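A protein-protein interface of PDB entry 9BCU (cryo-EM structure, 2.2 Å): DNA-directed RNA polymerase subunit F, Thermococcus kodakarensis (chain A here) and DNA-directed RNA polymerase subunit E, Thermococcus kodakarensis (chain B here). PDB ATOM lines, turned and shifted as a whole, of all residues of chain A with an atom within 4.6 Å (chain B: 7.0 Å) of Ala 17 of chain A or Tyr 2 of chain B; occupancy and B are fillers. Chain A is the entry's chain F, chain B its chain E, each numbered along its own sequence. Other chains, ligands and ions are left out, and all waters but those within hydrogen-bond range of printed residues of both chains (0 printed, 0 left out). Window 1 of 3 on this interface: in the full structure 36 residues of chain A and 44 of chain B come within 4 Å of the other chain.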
ATOM      1  N   HIS A  10      12.824 -32.035 -29.992  1.00  0.00           N
ATOM      2  CA  HIS A  10      13.618 -31.624 -28.845  1.00  0.00           C
ATOM      3  C   HIS A  10      12.705 -30.992 -27.805  1.00  0.00           C
ATOM      4  O   HIS A  10      11.743 -30.302 -28.152  1.00  0.00           O
ATOM      5  CB  HIS A  10      14.718 -30.636 -29.249  1.00  0.00           C
ATOM      6  CG  HIS A  10      15.885 -31.278 -29.934  1.00  0.00           C
ATOM      7  ND1 HIS A  10      16.175 -32.619 -29.809  1.00  0.00           N
ATOM      8  CD2 HIS A  10      16.834 -30.763 -30.750  1.00  0.00           C
ATOM      9  CE1 HIS A  10      17.252 -32.902 -30.518  1.00  0.00           C
ATOM     10  NE2 HIS A  10      17.672 -31.793 -31.099  1.00  0.00           N
ATOM     11  N   TYR A  11      13.016 -31.231 -26.535  1.00  0.00           N
ATOM     12  CA  TYR A  11      12.281 -30.650 -25.420  1.00  0.00           C
ATOM     13  C   TYR A  11      13.001 -29.387 -24.965  1.00  0.00           C
ATOM     14  O   TYR A  11      14.178 -29.439 -24.593  1.00  0.00           O
ATOM     15  CB  TYR A  11      12.156 -31.645 -24.267  1.00  0.00           C
ATOM     16  CG  TYR A  11      11.244 -32.814 -24.561  1.00  0.00           C
ATOM     17  CD1 TYR A  11       9.887 -32.751 -24.272  1.00  0.00           C
ATOM     18  CD2 TYR A  11      11.738 -33.981 -25.127  1.00  0.00           C
ATOM     19  CE1 TYR A  11       9.049 -33.816 -24.537  1.00  0.00           C
ATOM     20  CE2 TYR A  11      10.909 -35.053 -25.397  1.00  0.00           C
ATOM     21  CZ  TYR A  11       9.566 -34.965 -25.100  1.00  0.00           C
ATOM     22  OH  TYR A  11       8.735 -36.029 -25.367  1.00  0.00           O
ATOM     23  N   ILE A  12      12.296 -28.260 -24.994  1.00  0.00           N
ATOM     24  CA  ILE A  12      12.867 -26.977 -24.619  1.00  0.00           C
ATOM     25  C   ILE A  12      12.169 -26.472 -23.363  1.00  0.00           C
ATOM     26  O   ILE A  12      11.060 -26.891 -23.019  1.00  0.00           O
ATOM     27  CB  ILE A  12      12.767 -25.943 -25.758  1.00  0.00           C
ATOM     28  CG1 ILE A  12      11.309 -25.749 -26.177  1.00  0.00           C
ATOM     29  CG2 ILE A  12      13.613 -26.374 -26.945  1.00  0.00           C
ATOM     30  CD1 ILE A  12      10.929 -24.304 -26.401  1.00  0.00           C
ATOM     31  N   THR A  13      12.838 -25.555 -22.672  1.00  0.00           N
ATOM     32  CA  THR A  13      12.337 -25.012 -21.420  1.00  0.00           C
ATOM     33  C   THR A  13      11.415 -23.826 -21.698  1.00  0.00           C
ATOM     34  O   THR A  13      11.068 -23.529 -22.844  1.00  0.00           O
ATOM     35  CB  THR A  13      13.498 -24.618 -20.509  1.00  0.00           C
ATOM     36  OG1 THR A  13      13.893 -23.271 -20.796  1.00  0.00           O
ATOM     37  CG2 THR A  13      14.684 -25.545 -20.724  1.00  0.00           C
ATOM     38  N   ILE A  14      11.004 -23.136 -20.632  1.00  0.00           N
ATOM     39  CA  ILE A  14      10.114 -21.987 -20.774  1.00  0.00           C
ATOM     40  C   ILE A  14      10.839 -20.823 -21.444  1.00  0.00           C
ATOM     41  O   ILE A  14      10.254 -20.099 -22.257  1.00  0.00           O
ATOM     42  CB  ILE A  14       9.536 -21.602 -19.398  1.00  0.00           C
ATOM     43  CG1 ILE A  14       8.369 -22.523 -19.038  1.00  0.00           C
ATOM     44  CG2 ILE A  14       9.090 -20.143 -19.366  1.00  0.00           C
ATOM     45  CD1 ILE A  14       7.620 -22.114 -17.788  1.00  0.00           C
ATOM     46  N   ALA A  15      12.123 -20.635 -21.126  1.00  0.00           N
ATOM     47  CA  ALA A  15      12.861 -19.481 -21.637  1.00  0.00           C
ATOM     48  C   ALA A  15      13.051 -19.548 -23.150  1.00  0.00           C
ATOM     49  O   ALA A  15      12.967 -18.522 -23.837  1.00  0.00           O
ATOM     50  CB  ALA A  15      14.210 -19.373 -20.929  1.00  0.00           C
ATOM     51  N   GLU A  16      13.323 -20.740 -23.688  1.00  0.00           N
ATOM     52  CA  GLU A  16      13.455 -20.880 -25.137  1.00  0.00           C
ATOM     53  C   GLU A  16      12.137 -20.577 -25.839  1.00  0.00           C
ATOM     54  O   GLU A  16      12.118 -19.920 -26.888  1.00  0.00           O
ATOM     55  CB  GLU A  16      13.939 -22.286 -25.489  1.00  0.00           C
ATOM     56  CG  GLU A  16      15.387 -22.558 -25.117  1.00  0.00           C
ATOM     57  CD  GLU A  16      15.519 -23.279 -23.792  1.00  0.00           C
ATOM     58  OE1 GLU A  16      15.062 -22.729 -22.769  1.00  0.00           O
ATOM     59  OE2 GLU A  16      16.077 -24.396 -23.774  1.00  0.00           O
ATOM     60  N   ALA A  17      11.025 -21.050 -25.271  1.00  0.00           N
ATOM     61  CA  ALA A  17       9.715 -20.729 -25.823  1.00  0.00           C
ATOM     62  C   ALA A  17       9.441 -19.233 -25.747  1.00  0.00           C
ATOM     63  O   ALA A  17       8.839 -18.660 -26.659  1.00  0.00           O
ATOM     64  CB  ALA A  17       8.627 -21.513 -25.090  1.00  0.00           C
ATOM     65  N   LYS A  18       9.879 -18.588 -24.663  1.00  0.00           N
ATOM     66  CA  LYS A  18       9.733 -17.140 -24.542  1.00  0.00           C
ATOM     67  C   LYS A  18      10.511 -16.413 -25.628  1.00  0.00           C
ATOM     68  O   LYS A  18      10.008 -15.455 -26.226  1.00  0.00           O
ATOM     69  CB  LYS A  18      10.198 -16.682 -23.161  1.00  0.00           C
ATOM     70  CG  LYS A  18       9.597 -15.366 -22.703  1.00  0.00           C
ATOM     71  CD  LYS A  18      10.160 -14.951 -21.355  1.00  0.00           C
ATOM     72  CE  LYS A  18      11.506 -14.264 -21.507  1.00  0.00           C
ATOM     73  NZ  LYS A  18      11.447 -13.137 -22.478  1.00  0.00           N
ATOM     74  N   GLU A  19      11.742 -16.853 -25.895  1.00  0.00           N
ATOM     75  CA  GLU A  19      12.542 -16.226 -26.944  1.00  0.00           C
ATOM     76  C   GLU A  19      11.905 -16.420 -28.317  1.00  0.00           C
ATOM     77  O   GLU A  19      11.840 -15.480 -29.120  1.00  0.00           O
ATOM     78  CB  GLU A  19      13.963 -16.790 -26.926  1.00  0.00           C
ATOM     79  CG  GLU A  19      15.007 -15.858 -27.520  1.00  0.00           C
ATOM     80  CD  GLU A  19      16.405 -16.441 -27.466  1.00  0.00           C
ATOM     81  OE1 GLU A  19      16.532 -17.673 -27.303  1.00  0.00           O
ATOM     82  OE2 GLU A  19      17.378 -15.667 -27.586  1.00  0.00           O
ATOM     83  N   LEU A  20      11.421 -17.633 -28.597  1.00  0.00           N
ATOM     84  CA  LEU A  20      10.779 -17.895 -29.884  1.00  0.00           C
ATOM     85  C   LEU A  20       9.499 -17.081 -30.041  1.00  0.00           C
ATOM     86  O   LEU A  20       9.223 -16.543 -31.121  1.00  0.00           O
ATOM     87  CB  LEU A  20      10.491 -19.388 -30.031  1.00  0.00           C
ATOM     88  CG  LEU A  20      11.717 -20.300 -30.109  1.00  0.00           C
ATOM     89  CD1 LEU A  20      11.303 -21.763 -30.103  1.00  0.00           C
ATOM     90  CD2 LEU A  20      12.554 -19.979 -31.336  1.00  0.00           C
ATOM     91  N   LEU A  21       8.708 -16.970 -28.971  1.00  0.00           N
ATOM     92  CA  LEU A  21       7.483 -16.183 -29.031  1.00  0.00           C
ATOM     93  C   LEU A  21       7.775 -14.696 -29.169  1.00  0.00           C
ATOM     94  O   LEU A  21       7.026 -13.986 -29.842  1.00  0.00           O
ATOM     95  CB  LEU A  21       6.627 -16.451 -27.793  1.00  0.00           C
ATOM     96  CG  LEU A  21       5.849 -17.769 -27.804  1.00  0.00           C
ATOM     97  CD1 LEU A  21       5.525 -18.220 -26.388  1.00  0.00           C
ATOM     98  CD2 LEU A  21       4.582 -17.641 -28.634  1.00  0.00           C
ATOM     99  N   SER A  44       0.529 -17.496 -24.350  1.00  0.00           N
ATOM    100  CA  SER A  44       1.737 -18.255 -24.037  1.00  0.00           C
ATOM    101  C   SER A  44       2.925 -17.333 -23.798  1.00  0.00           C
ATOM    102  O   SER A  44       3.725 -17.566 -22.883  1.00  0.00           O
ATOM    103  CB  SER A  44       2.043 -19.239 -25.166  1.00  0.00           C
ATOM    104  OG  SER A  44       1.268 -20.416 -25.039  1.00  0.00           O
ATOM    105  N   MET B   1       4.242 -28.802 -21.819  1.00  0.00           N
ATOM    106  CA  MET B   1       5.594 -29.177 -22.215  1.00  0.00           C
ATOM    107  C   MET B   1       5.941 -28.621 -23.592  1.00  0.00           C
ATOM    108  O   MET B   1       5.464 -29.123 -24.610  1.00  0.00           O
ATOM    109  CB  MET B   1       5.752 -30.698 -22.206  1.00  0.00           C
ATOM    110  CG  MET B   1       7.193 -31.170 -22.291  1.00  0.00           C
ATOM    111  SD  MET B   1       8.320 -30.142 -21.330  1.00  0.00           S
ATOM    112  CE  MET B   1       8.490 -31.126 -19.844  1.00  0.00           C
ATOM    113  N   TYR B   2       6.769 -27.580 -23.613  1.00  0.00           N
ATOM    114  CA  TYR B   2       7.202 -26.994 -24.873  1.00  0.00           C
ATOM    115  C   TYR B   2       8.126 -27.949 -25.616  1.00  0.00           C
ATOM    116  O   TYR B   2       9.011 -28.572 -25.022  1.00  0.00           O
ATOM    117  CB  TYR B   2       7.913 -25.665 -24.623  1.00  0.00           C
ATOM    118  CG  TYR B   2       6.991 -24.546 -24.196  1.00  0.00           C
ATOM    119  CD1 TYR B   2       6.039 -24.034 -25.067  1.00  0.00           C
ATOM    120  CD2 TYR B   2       7.075 -23.999 -22.923  1.00  0.00           C
ATOM    121  CE1 TYR B   2       5.197 -23.009 -24.683  1.00  0.00           C
ATOM    122  CE2 TYR B   2       6.236 -22.974 -22.529  1.00  0.00           C
ATOM    123  CZ  TYR B   2       5.299 -22.484 -23.413  1.00  0.00           C
ATOM    124  OH  TYR B   2       4.460 -21.463 -23.025  1.00  0.00           O
ATOM    125  N   LYS B   3       7.917 -28.063 -26.926  1.00  0.00           N
ATOM    126  CA  LYS B   3       8.718 -28.944 -27.761  1.00  0.00           C
ATOM    127  C   LYS B   3       9.082 -28.231 -29.054  1.00  0.00           C
ATOM    128  O   LYS B   3       8.326 -27.394 -29.555  1.00  0.00           O
ATOM    129  CB  LYS B   3       7.980 -30.252 -28.078  1.00  0.00           C
ATOM    130  CG  LYS B   3       7.903 -31.223 -26.913  1.00  0.00           C
ATOM    131  CD  LYS B   3       6.946 -32.365 -27.211  1.00  0.00           C
ATOM    132  CE  LYS B   3       7.469 -33.241 -28.338  1.00  0.00           C
ATOM    133  NZ  LYS B   3       6.636 -34.460 -28.526  1.00  0.00           N
ATOM    134  N   LEU B   4      10.253 -28.572 -29.587  1.00  0.00           N
ATOM    135  CA  LEU B   4      10.729 -28.053 -30.864  1.00  0.00           C
ATOM    136  C   LEU B   4      10.921 -29.225 -31.814  1.00  0.00           C
ATOM    137  O   LEU B   4      11.668 -30.159 -31.505  1.00  0.00           O
ATOM    138  CB  LEU B   4      12.036 -27.277 -30.689  1.00  0.00           C
ATOM    139  CG  LEU B   4      12.395 -26.293 -31.803  1.00  0.00           C
ATOM    140  CD1 LEU B   4      11.433 -25.118 -31.807  1.00  0.00           C
ATOM    141  CD2 LEU B   4      13.830 -25.815 -31.653  1.00  0.00           C
ATOM    142  N   LEU B  46       1.935 -23.726 -31.799  1.00  0.00           N
ATOM    143  CA  LEU B  46       2.067 -22.340 -31.374  1.00  0.00           C
ATOM    144  C   LEU B  46       2.533 -21.427 -32.502  1.00  0.00           C
ATOM    145  O   LEU B  46       1.883 -20.417 -32.792  1.00  0.00           O
ATOM    146  CB  LEU B  46       3.028 -22.244 -30.186  1.00  0.00           C
ATOM    147  CG  LEU B  46       2.405 -22.453 -28.805  1.00  0.00           C
ATOM    148  CD1 LEU B  46       3.450 -22.280 -27.719  1.00  0.00           C
ATOM    149  CD2 LEU B  46       1.243 -21.498 -28.591  1.00  0.00           C
ATOM    150  N   LEU B  75       7.323 -24.806 -33.129  1.00  0.00           N
ATOM    151  CA  LEU B  75       7.284 -24.752 -31.675  1.00  0.00           C
ATOM    152  C   LEU B  75       5.890 -25.164 -31.218  1.00  0.00           C
ATOM    153  O   LEU B  75       4.897 -24.543 -31.611  1.00  0.00           O
ATOM    154  CB  LEU B  75       7.630 -23.353 -31.167  1.00  0.00           C
ATOM    155  CG  LEU B  75       7.201 -23.026 -29.735  1.00  0.00           C
ATOM    156  CD1 LEU B  75       8.061 -23.777 -28.732  1.00  0.00           C
ATOM    157  CD2 LEU B  75       7.260 -21.528 -29.482  1.00  0.00           C
ATOM    158  N   VAL B  76       5.817 -26.212 -30.398  1.00  0.00           N
ATOM    159  CA  VAL B  76       4.544 -26.771 -29.966  1.00  0.00           C
ATOM    160  C   VAL B  76       4.545 -26.939 -28.453  1.00  0.00           C
ATOM    161  O   VAL B  76       5.593 -27.032 -27.811  1.00  0.00           O
ATOM    162  CB  VAL B  76       4.235 -28.122 -30.648  1.00  0.00           C
ATOM    163  CG1 VAL B  76       3.922 -27.917 -32.122  1.00  0.00           C
ATOM    164  CG2 VAL B  76       5.399 -29.081 -30.472  1.00  0.00           C
ATOM    165  N   TRP B  77       3.340 -26.973 -27.889  1.00  0.00           N
ATOM    166  CA  TRP B  77       3.127 -27.212 -26.467  1.00  0.00           C
ATOM    167  C   TRP B  77       2.149 -28.366 -26.325  1.00  0.00           C
ATOM    168  O   TRP B  77       1.035 -28.304 -26.855  1.00  0.00           O
ATOM    169  CB  TRP B  77       2.594 -25.958 -25.769  1.00  0.00           C
ATOM    170  CG  TRP B  77       2.554 -26.059 -24.275  1.00  0.00           C
ATOM    171  CD1 TRP B  77       3.551 -25.730 -23.405  1.00  0.00           C
ATOM    172  CD2 TRP B  77       1.456 -26.512 -23.474  1.00  0.00           C
ATOM    173  NE1 TRP B  77       3.144 -25.953 -22.112  1.00  0.00           N
ATOM    174  CE2 TRP B  77       1.861 -26.433 -22.128  1.00  0.00           C
ATOM    175  CE3 TRP B  77       0.170 -26.979 -23.765  1.00  0.00           C
ATOM    176  CZ2 TRP B  77       1.028 -26.804 -21.074  1.00  0.00           C
ATOM    177  CZ3 TRP B  77      -0.656 -27.345 -22.718  1.00  0.00           C
ATOM    178  CH2 TRP B  77      -0.223 -27.256 -21.389  1.00  0.00           C
ATOM    179  N   GLU B  78       2.558 -29.414 -25.615  1.00  0.00           N
ATOM    180  CA  GLU B  78       1.751 -30.620 -25.478  1.00  0.00           C
ATOM    181  C   GLU B  78       1.533 -30.941 -24.007  1.00  0.00           C
ATOM    182  O   GLU B  78       2.513 -31.115 -23.263  1.00  0.00           O
ATOM    183  CB  GLU B  78       2.420 -31.801 -26.185  1.00  0.00           C
ATOM    184  CG  GLU B  78       1.657 -33.109 -26.058  1.00  0.00           C
ATOM    185  CD  GLU B  78       2.531 -34.321 -26.315  1.00  0.00           C
ATOM    186  OE1 GLU B  78       3.535 -34.493 -25.594  1.00  0.00           O
ATOM    187  OE2 GLU B  78       2.212 -35.101 -27.237  1.00  0.00           O
ATOM    188  N   GLU B  83       1.743 -34.796 -15.387  1.00  0.00           N
ATOM    189  CA  GLU B  83       2.777 -33.798 -15.617  1.00  0.00           C
ATOM    190  C   GLU B  83       2.522 -32.589 -14.727  1.00  0.00           C
ATOM    191  O   GLU B  83       1.428 -32.017 -14.748  1.00  0.00           O
ATOM    192  CB  GLU B  83       2.817 -33.375 -17.088  1.00  0.00           C
ATOM    193  CG  GLU B  83       3.952 -32.425 -17.428  1.00  0.00           C
ATOM    194  CD  GLU B  83       3.611 -31.498 -18.579  1.00  0.00           C
ATOM    195  OE1 GLU B  83       2.502 -31.625 -19.138  1.00  0.00           O
ATOM    196  OE2 GLU B  83       4.454 -30.644 -18.925  1.00  0.00           O
ATOM    197  N   ILE B 101      -1.730 -22.156 -17.464  1.00  0.00           N
ATOM    198  CA  ILE B 101      -0.451 -22.855 -17.458  1.00  0.00           C
ATOM    199  C   ILE B 101       0.267 -22.756 -18.791  1.00  0.00           C
ATOM    200  O   ILE B 101       1.346 -23.347 -18.948  1.00  0.00           O
ATOM    201  CB  ILE B 101      -0.623 -24.331 -17.054  1.00  0.00           C
ATOM    202  CG1 ILE B 101      -1.291 -25.119 -18.183  1.00  0.00           C
ATOM    203  CG2 ILE B 101      -1.434 -24.439 -15.773  1.00  0.00           C
ATOM    204  CD1 ILE B 101      -1.506 -26.582 -17.864  1.00  0.00           C
ATOM    205  N   GLY B 102      -0.289 -22.027 -19.754  1.00  0.00           N
ATOM    206  CA  GLY B 102       0.299 -21.903 -21.065  1.00  0.00           C
ATOM    207  C   GLY B 102      -0.744 -21.529 -22.096  1.00  0.00           C
ATOM    208  O   GLY B 102      -1.611 -20.685 -21.852  1.00  0.00           O
ATOM    209  N   PRO B 103      -0.683 -22.154 -23.275  1.00  0.00           N
ATOM    210  CA  PRO B 103      -1.712 -21.890 -24.293  1.00  0.00           C
ATOM    211  C   PRO B 103      -3.093 -22.387 -23.901  1.00  0.00           C
ATOM    212  O   PRO B 103      -4.084 -21.929 -24.482  1.00  0.00           O
ATOM    213  CB  PRO B 103      -1.182 -22.626 -25.530  1.00  0.00           C
ATOM    214  CG  PRO B 103      -0.318 -23.703 -24.983  1.00  0.00           C
ATOM    215  CD  PRO B 103       0.278 -23.184 -23.704  1.00  0.00           C
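The backbone carbonyl oxygen (O) of Tyr 2 of chain B is in hydrogen-bond range of the backbone NH (N) of Ile 12 of chain A (3.3 Å). N of His 10 of chain A sits at hydrogen-bond distance from O of Leu 4 of chain B, at 2.7 Å. OG of Ser 44 of chain A lies close to N of Pro 103 of chain B (3.2 Å).
The backbone carbonyl oxygen (O) of Met 1 of chain B is in hydrogen-bond range of the backbone NH (N) of Glu 78 of chain B, at 3.1 Å. The backbone NH (N) of Leu 46 of chain B sits at hydrogen-bond distance from the backbone carbonyl oxygen (O) of Leu 75 of chain B, 3.1 Å away. N of Met 1 of chain B sits at hydrogen-bond distance from OE2 of Glu 83 of chain B. N of Lys 3 of chain B lies within hydrogen-bond range of O of Val 76 of chain B, 2.7 Å away.
Of the printed residues of chain B, Ala 17 of chain A touches Tyr 2. Of the printed residues of chain A, Lys 3 of chain B touches His 10 (3.3 Å) and Tyr 11 (3.6 Å). Of the printed residues of chain A, Met 1 of chain B touches Tyr 11. Of the printed residues of chain B, Leu 20 of chain A touches Leu 4 (3.8 Å) and Leu 75 (3.9 Å). Ile 101 of chain B touches none of the printed residues of chain A. Glu 78 of chain B touches none of the printed residues of chain A.
Lys 3 of chain B touches His 10 of chain A (CA to O, 3.3 Å). Tyr 11 of chain A touches Met 1 of chain B (CD1 to CG, 3.7 Å). Tyr 2 of chain B touches Tyr 11 of chain A (O to CA, 3.9 Å). Tyr 11 of chain A touches Lys 3 of chain B (CD1 to CG, 3.6 Å). Ile 12 of chain A touches Leu 75 of chain B (CD1 to CD1, 3.7 Å). Tyr 2 of chain B touches Ala 17 of chain A. CB of Leu 20 of chain A touches CD2 of Leu 75 of chain B, at 3.9 Å. Ser 44 of chain A touches Tyr 2 of chain B (OG to OH, 3.9 Å). Leu 46 of chain B touches Ser 44 of chain A. C of Gly 102 of chain B touches OG of Ser 44 of chain A, 3.7 Å away.
Hydrophobic or aromatic side chains of chain A within 4 Å of the printed part of chain B: His 10, Tyr 11, Ile 12, Ala 17 and Leu 20. Of the 13 printed residues of chain B, 8 touch a printed residue of chain A. Hydrophobic or aromatic side chains of chain B that line the printed part of chain A: Met 1, Tyr 2, Leu 4, Leu 46, Leu 75 and Pro 103. Among the printed residues, 14 pairs touch across the chains. Among the printed residues, no Asp or Glu carboxylate lies within 4 Å of a Lys or Arg side-chain nitrogen of the other chain.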
